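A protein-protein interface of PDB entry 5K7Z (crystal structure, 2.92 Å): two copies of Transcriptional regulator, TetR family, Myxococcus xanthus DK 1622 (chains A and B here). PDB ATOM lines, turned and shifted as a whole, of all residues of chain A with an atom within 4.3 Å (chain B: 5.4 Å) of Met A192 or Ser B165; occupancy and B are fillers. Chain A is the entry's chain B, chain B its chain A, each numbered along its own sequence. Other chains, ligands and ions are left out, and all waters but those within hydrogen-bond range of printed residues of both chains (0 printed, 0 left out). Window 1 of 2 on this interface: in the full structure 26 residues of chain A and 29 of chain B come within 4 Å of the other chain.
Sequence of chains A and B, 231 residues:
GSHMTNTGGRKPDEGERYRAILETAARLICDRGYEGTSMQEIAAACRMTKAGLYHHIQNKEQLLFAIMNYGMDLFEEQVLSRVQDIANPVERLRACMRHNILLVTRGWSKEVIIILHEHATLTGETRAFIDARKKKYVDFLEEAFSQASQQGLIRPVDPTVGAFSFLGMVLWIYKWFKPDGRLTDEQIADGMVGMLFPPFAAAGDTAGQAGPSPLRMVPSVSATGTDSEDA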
ATOM      1  N   MET A  97     -26.755  31.819  21.443  1.00  0.00           N
ATOM      2  CA  MET A  97     -25.844  31.342  20.409  1.00  0.00           C
ATOM      3  C   MET A  97     -26.540  30.370  19.468  1.00  0.00           C
ATOM      4  O   MET A  97     -26.379  30.452  18.247  1.00  0.00           O
ATOM      5  CB  MET A  97     -24.626  30.677  21.051  1.00  0.00           C
ATOM      6  CG  MET A  97     -23.650  30.068  20.060  1.00  0.00           C
ATOM      7  SD  MET A  97     -22.116  29.517  20.827  1.00  0.00           S
ATOM      8  CE  MET A  97     -21.285  31.072  21.102  1.00  0.00           C
ATOM      9  N   ILE A 101     -27.103  31.290  15.444  1.00  0.00           N
ATOM     10  CA  ILE A 101     -26.461  30.481  14.412  1.00  0.00           C
ATOM     11  C   ILE A 101     -27.491  29.978  13.410  1.00  0.00           C
ATOM     12  O   ILE A 101     -27.253  29.988  12.197  1.00  0.00           O
ATOM     13  CB  ILE A 101     -25.682  29.318  15.057  1.00  0.00           C
ATOM     14  CG1 ILE A 101     -24.505  29.861  15.870  1.00  0.00           C
ATOM     15  CG2 ILE A 101     -25.180  28.342  13.996  1.00  0.00           C
ATOM     16  CD1 ILE A 101     -23.823  28.827  16.739  1.00  0.00           C
ATOM     17  N   MET A 169     -17.773  34.188  16.397  1.00  0.00           N
ATOM     18  CA  MET A 169     -18.019  32.789  16.065  1.00  0.00           C
ATOM     19  C   MET A 169     -19.291  32.633  15.244  1.00  0.00           C
ATOM     20  O   MET A 169     -19.297  31.959  14.209  1.00  0.00           O
ATOM     21  CB  MET A 169     -18.127  31.954  17.341  1.00  0.00           C
ATOM     22  CG  MET A 169     -16.841  31.759  18.107  1.00  0.00           C
ATOM     23  SD  MET A 169     -17.136  30.694  19.526  1.00  0.00           S
ATOM     24  CE  MET A 169     -15.535  30.729  20.319  1.00  0.00           C
ATOM     25  N   ILE A 188     -22.841  22.270  14.088  1.00  0.00           N
ATOM     26  CA  ILE A 188     -21.991  23.437  14.300  1.00  0.00           C
ATOM     27  C   ILE A 188     -22.418  24.179  15.557  1.00  0.00           C
ATOM     28  O   ILE A 188     -21.580  24.657  16.330  1.00  0.00           O
ATOM     29  CB  ILE A 188     -22.023  24.352  13.061  1.00  0.00           C
ATOM     30  CG1 ILE A 188     -21.438  23.618  11.852  1.00  0.00           C
ATOM     31  CG2 ILE A 188     -21.244  25.640  13.320  1.00  0.00           C
ATOM     32  CD1 ILE A 188     -21.625  24.339  10.538  1.00  0.00           C
ATOM     33  N   ALA A 189     -23.727  24.288  15.784  1.00  0.00           N
ATOM     34  CA  ALA A 189     -24.221  24.959  16.981  1.00  0.00           C
ATOM     35  C   ALA A 189     -23.757  24.235  18.238  1.00  0.00           C
ATOM     36  O   ALA A 189     -23.105  24.824  19.106  1.00  0.00           O
ATOM     37  CB  ALA A 189     -25.746  25.050  16.935  1.00  0.00           C
ATOM     38  N   ASP A 190     -24.077  22.943  18.347  1.00  0.00           N
ATOM     39  CA  ASP A 190     -23.673  22.175  19.520  1.00  0.00           C
ATOM     40  C   ASP A 190     -22.169  22.259  19.745  1.00  0.00           C
ATOM     41  O   ASP A 190     -21.707  22.342  20.888  1.00  0.00           O
ATOM     42  CB  ASP A 190     -24.105  20.717  19.367  1.00  0.00           C
ATOM     43  CG  ASP A 190     -25.609  20.562  19.235  1.00  0.00           C
ATOM     44  OD1 ASP A 190     -26.319  20.742  20.246  1.00  0.00           O
ATOM     45  OD2 ASP A 190     -26.080  20.249  18.122  1.00  0.00           O
ATOM     46  N   GLY A 191     -21.388  22.245  18.665  1.00  0.00           N
ATOM     47  CA  GLY A 191     -19.943  22.281  18.810  1.00  0.00           C
ATOM     48  C   GLY A 191     -19.434  23.611  19.331  1.00  0.00           C
ATOM     49  O   GLY A 191     -18.534  23.653  20.173  1.00  0.00           O
ATOM     50  N   MET A 192     -19.999  24.716  18.837  1.00  0.00           N
ATOM     51  CA  MET A 192     -19.553  26.033  19.279  1.00  0.00           C
ATOM     52  C   MET A 192     -20.021  26.330  20.697  1.00  0.00           C
ATOM     53  O   MET A 192     -19.278  26.918  21.491  1.00  0.00           O
ATOM     54  CB  MET A 192     -20.055  27.107  18.315  1.00  0.00           C
ATOM     55  CG  MET A 192     -19.201  27.268  17.071  1.00  0.00           C
ATOM     56  SD  MET A 192     -19.840  28.528  15.957  1.00  0.00           S
ATOM     57  CE  MET A 192     -18.573  28.535  14.693  1.00  0.00           C
ATOM     58  N   VAL A 193     -21.251  25.936  21.033  1.00  0.00           N
ATOM     59  CA  VAL A 193     -21.765  26.171  22.380  1.00  0.00           C
ATOM     60  C   VAL A 193     -20.865  25.501  23.409  1.00  0.00           C
ATOM     61  O   VAL A 193     -20.426  26.127  24.379  1.00  0.00           O
ATOM     62  CB  VAL A 193     -23.220  25.678  22.493  1.00  0.00           C
ATOM     63  CG1 VAL A 193     -23.715  25.773  23.929  1.00  0.00           C
ATOM     64  CG2 VAL A 193     -24.125  26.486  21.577  1.00  0.00           C
ATOM     65  N   GLY A 194     -20.575  24.214  23.210  1.00  0.00           N
ATOM     66  CA  GLY A 194     -19.704  23.511  24.132  1.00  0.00           C
ATOM     67  C   GLY A 194     -18.281  24.024  24.108  1.00  0.00           C
ATOM     68  O   GLY A 194     -17.553  23.894  25.096  1.00  0.00           O
ATOM     69  N   MET A 195     -17.864  24.617  22.991  1.00  0.00           N
ATOM     70  CA  MET A 195     -16.493  25.094  22.862  1.00  0.00           C
ATOM     71  C   MET A 195     -16.271  26.386  23.637  1.00  0.00           C
ATOM     72  O   MET A 195     -15.210  26.573  24.242  1.00  0.00           O
ATOM     73  CB  MET A 195     -16.151  25.291  21.387  1.00  0.00           C
ATOM     74  CG  MET A 195     -14.862  26.050  21.146  1.00  0.00           C
ATOM     75  SD  MET A 195     -14.138  25.674  19.546  1.00  0.00           S
ATOM     76  CE  MET A 195     -12.850  24.539  20.040  1.00  0.00           C
ATOM     77  N   LEU A 196     -17.253  27.286  23.632  1.00  0.00           N
ATOM     78  CA  LEU A 196     -17.142  28.555  24.338  1.00  0.00           C
ATOM     79  C   LEU A 196     -17.807  28.538  25.706  1.00  0.00           C
ATOM     80  O   LEU A 196     -17.350  29.241  26.612  1.00  0.00           O
ATOM     81  CB  LEU A 196     -17.753  29.682  23.498  1.00  0.00           C
ATOM     82  CG  LEU A 196     -17.633  31.098  24.064  1.00  0.00           C
ATOM     83  CD1 LEU A 196     -16.180  31.511  24.195  1.00  0.00           C
ATOM     84  CD2 LEU A 196     -18.384  32.092  23.195  1.00  0.00           C
ATOM     85  N   THR B 160     -13.158  21.150  12.285  1.00  0.00           N
ATOM     86  CA  THR B 160     -13.745  22.216  11.479  1.00  0.00           C
ATOM     87  C   THR B 160     -14.433  23.250  12.362  1.00  0.00           C
ATOM     88  O   THR B 160     -14.258  24.458  12.172  1.00  0.00           O
ATOM     89  CB  THR B 160     -14.732  21.627  10.469  1.00  0.00           C
ATOM     90  OG1 THR B 160     -14.039  20.744   9.581  1.00  0.00           O
ATOM     91  CG2 THR B 160     -15.402  22.728   9.655  1.00  0.00           C
ATOM     92  N   VAL B 161     -15.223  22.793  13.335  1.00  0.00           N
ATOM     93  CA  VAL B 161     -15.891  23.717  14.245  1.00  0.00           C
ATOM     94  C   VAL B 161     -14.869  24.534  15.019  1.00  0.00           C
ATOM     95  O   VAL B 161     -15.120  25.695  15.361  1.00  0.00           O
ATOM     96  CB  VAL B 161     -16.831  22.946  15.192  1.00  0.00           C
ATOM     97  CG1 VAL B 161     -17.501  23.896  16.177  1.00  0.00           C
ATOM     98  CG2 VAL B 161     -17.877  22.181  14.394  1.00  0.00           C
ATOM     99  N   GLY B 162     -13.709  23.954  15.307  1.00  0.00           N
ATOM    100  CA  GLY B 162     -12.676  24.663  16.032  1.00  0.00           C
ATOM    101  C   GLY B 162     -11.943  25.660  15.164  1.00  0.00           C
ATOM    102  O   GLY B 162     -11.554  26.734  15.631  1.00  0.00           O
ATOM    103  N   ALA B 163     -11.746  25.314  13.890  1.00  0.00           N
ATOM    104  CA  ALA B 163     -11.046  26.213  12.981  1.00  0.00           C
ATOM    105  C   ALA B 163     -11.857  27.476  12.720  1.00  0.00           C
ATOM    106  O   ALA B 163     -11.312  28.584  12.743  1.00  0.00           O
ATOM    107  CB  ALA B 163     -10.737  25.499  11.668  1.00  0.00           C
ATOM    108  N   PHE B 164     -13.160  27.332  12.474  1.00  0.00           N
ATOM    109  CA  PHE B 164     -13.997  28.487  12.178  1.00  0.00           C
ATOM    110  C   PHE B 164     -14.425  29.238  13.429  1.00  0.00           C
ATOM    111  O   PHE B 164     -14.849  30.393  13.326  1.00  0.00           O
ATOM    112  CB  PHE B 164     -15.220  28.050  11.378  1.00  0.00           C
ATOM    113  CG  PHE B 164     -14.900  27.669   9.961  1.00  0.00           C
ATOM    114  CD1 PHE B 164     -14.492  28.627   9.052  1.00  0.00           C
ATOM    115  CD2 PHE B 164     -15.001  26.357   9.540  1.00  0.00           C
ATOM    116  CE1 PHE B 164     -14.194  28.285   7.753  1.00  0.00           C
ATOM    117  CE2 PHE B 164     -14.704  26.012   8.239  1.00  0.00           C
ATOM    118  CZ  PHE B 164     -14.301  26.977   7.347  1.00  0.00           C
ATOM    119  N   SER B 165     -14.330  28.616  14.604  1.00  0.00           N
ATOM    120  CA  SER B 165     -14.432  29.376  15.844  1.00  0.00           C
ATOM    121  C   SER B 165     -13.166  30.187  16.072  1.00  0.00           C
ATOM    122  O   SER B 165     -13.228  31.343  16.501  1.00  0.00           O
ATOM    123  CB  SER B 165     -14.686  28.432  17.019  1.00  0.00           C
ATOM    124  OG  SER B 165     -15.830  27.630  16.795  1.00  0.00           O
ATOM    125  N   PHE B 166     -12.008  29.591  15.786  1.00  0.00           N
ATOM    126  CA  PHE B 166     -10.754  30.332  15.801  1.00  0.00           C
ATOM    127  C   PHE B 166     -10.821  31.525  14.859  1.00  0.00           C
ATOM    128  O   PHE B 166     -10.463  32.648  15.228  1.00  0.00           O
ATOM    129  CB  PHE B 166      -9.607  29.397  15.410  1.00  0.00           C
ATOM    130  CG  PHE B 166      -8.252  30.048  15.410  1.00  0.00           C
ATOM    131  CD1 PHE B 166      -7.851  30.852  14.359  1.00  0.00           C
ATOM    132  CD2 PHE B 166      -7.372  29.831  16.449  1.00  0.00           C
ATOM    133  CE1 PHE B 166      -6.607  31.445  14.356  1.00  0.00           C
ATOM    134  CE2 PHE B 166      -6.126  30.417  16.450  1.00  0.00           C
ATOM    135  CZ  PHE B 166      -5.744  31.227  15.403  1.00  0.00           C
ATOM    136  N   LEU B 167     -11.291  31.296  13.632  1.00  0.00           N
ATOM    137  CA  LEU B 167     -11.316  32.353  12.628  1.00  0.00           C
ATOM    138  C   LEU B 167     -12.394  33.382  12.932  1.00  0.00           C
ATOM    139  O   LEU B 167     -12.177  34.585  12.752  1.00  0.00           O
ATOM    140  CB  LEU B 167     -11.528  31.740  11.247  1.00  0.00           C
ATOM    141  CG  LEU B 167     -10.388  30.835  10.777  1.00  0.00           C
ATOM    142  CD1 LEU B 167     -10.850  29.918   9.669  1.00  0.00           C
ATOM    143  CD2 LEU B 167      -9.207  31.670  10.323  1.00  0.00           C
ATOM    144  N   GLY B 168     -13.561  32.934  13.387  1.00  0.00           N
ATOM    145  CA  GLY B 168     -14.632  33.839  13.750  1.00  0.00           C
ATOM    146  C   GLY B 168     -14.184  34.909  14.721  1.00  0.00           C
ATOM    147  O   GLY B 168     -14.276  36.103  14.428  1.00  0.00           O
ATOM    148  N   MET B 169     -13.691  34.489  15.886  1.00  0.00           N
ATOM    149  CA  MET B 169     -13.206  35.443  16.878  1.00  0.00           C
ATOM    150  C   MET B 169     -12.162  36.373  16.280  1.00  0.00           C
ATOM    151  O   MET B 169     -12.227  37.596  16.447  1.00  0.00           O
ATOM    152  CB  MET B 169     -12.611  34.698  18.072  1.00  0.00           C
ATOM    153  CG  MET B 169     -13.577  33.805  18.822  1.00  0.00           C
ATOM    154  SD  MET B 169     -12.748  32.778  20.048  1.00  0.00           S
ATOM    155  CE  MET B 169     -11.811  33.987  20.969  1.00  0.00           C
ATOM    156  N   VAL B 170     -11.189  35.803  15.572  1.00  0.00           N
ATOM    157  CA  VAL B 170     -10.008  36.560  15.172  1.00  0.00           C
ATOM    158  C   VAL B 170     -10.338  37.502  14.021  1.00  0.00           C
ATOM    159  O   VAL B 170     -10.007  38.692  14.061  1.00  0.00           O
ATOM    160  CB  VAL B 170      -8.867  35.591  14.808  1.00  0.00           C
ATOM    161  CG1 VAL B 170      -7.668  36.339  14.248  1.00  0.00           C
ATOM    162  CG2 VAL B 170      -8.463  34.785  16.030  1.00  0.00           C
ATOM    163  N   LEU B 196     -10.467  30.480  24.674  1.00  0.00           N
ATOM    164  CA  LEU B 196     -10.582  29.290  23.842  1.00  0.00           C
ATOM    165  C   LEU B 196      -9.459  28.290  24.067  1.00  0.00           C
ATOM    166  O   LEU B 196      -9.667  27.093  23.864  1.00  0.00           O
ATOM    167  CB  LEU B 196     -10.616  29.685  22.361  1.00  0.00           C
ATOM    168  CG  LEU B 196     -11.351  28.729  21.422  1.00  0.00           C
ATOM    169  CD1 LEU B 196     -12.009  29.504  20.301  1.00  0.00           C
ATOM    170  CD2 LEU B 196     -10.408  27.692  20.847  1.00  0.00           C
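Met B169 touches its own counterpart, Met A169. Met A169 touches Leu B196, but with the chains exchanged Leu A196 does not touch Met B169 (5.5 Å). 2 positions are printed for both chains. Of the 8 pairs that touch across the chains among the printed residues, 1 has its exchanged pair printed and touching as well.
OG of Ser B165 sits at hydrogen-bond distance from O of Val B161, 2.5 Å away.
Printed residues of chain B within 4 Å of Met A169: Ser B165 (3.98 Å), Met B169 (3.5 Å) and Leu B196 (3.7 Å). Of the printed residues of chain B, Met A192 touches Val B161 and Ser B165. Printed residues of chain B within 4 Å of Met A195: Gly B162 and Ser B165. Printed residues of chain A within 4 Å of Val B161: Gly A191 (3.7 Å) and Met A192 (3.7 Å). Of the printed residues of chain A, Met B169 touches Met A169 (3.5 Å). The nearest residue of chain B that does not touch Met A192 is Phe B164 (4.4 Å). The nearest printed residue of chain B that does not touch Met A169 is Gly B168 (4.03 Å).
The side-chain hydroxyl (OG) of Ser B165 lies within hydrogen-bond range of the side-chain sulfur (SD) of Met A195.
Hydrophobic or aromatic side chains of chain B that line the printed part of chain A: Val B161, Met B169 and Leu B196. Hydrophobic or aromatic side chains of chain A that line the printed part of chain B: Met A169, Met A192 and Met A195. Along chain A the printed residues that touch a printed residue of chain B span positions 169 to 195. Among the printed residues, no Asp or Glu carboxylate lies within 4 Å of a Lys or Arg side-chain nitrogen of the other chain.
CG of Met A169 touches O of Ser B165, at 3.98 Å. CE of Met A169 touches SD of Met B169, 3.5 Å away. Leu B196 touches Met A169 (CD1 to CE, 3.7 Å). Gly A191 touches Val B161 (C to CG1, 3.7 Å). Met A192 touches Val B161. Met A192 touches Ser B165 (CG to OG, 3.4 Å). Met A195 touches Gly B162.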
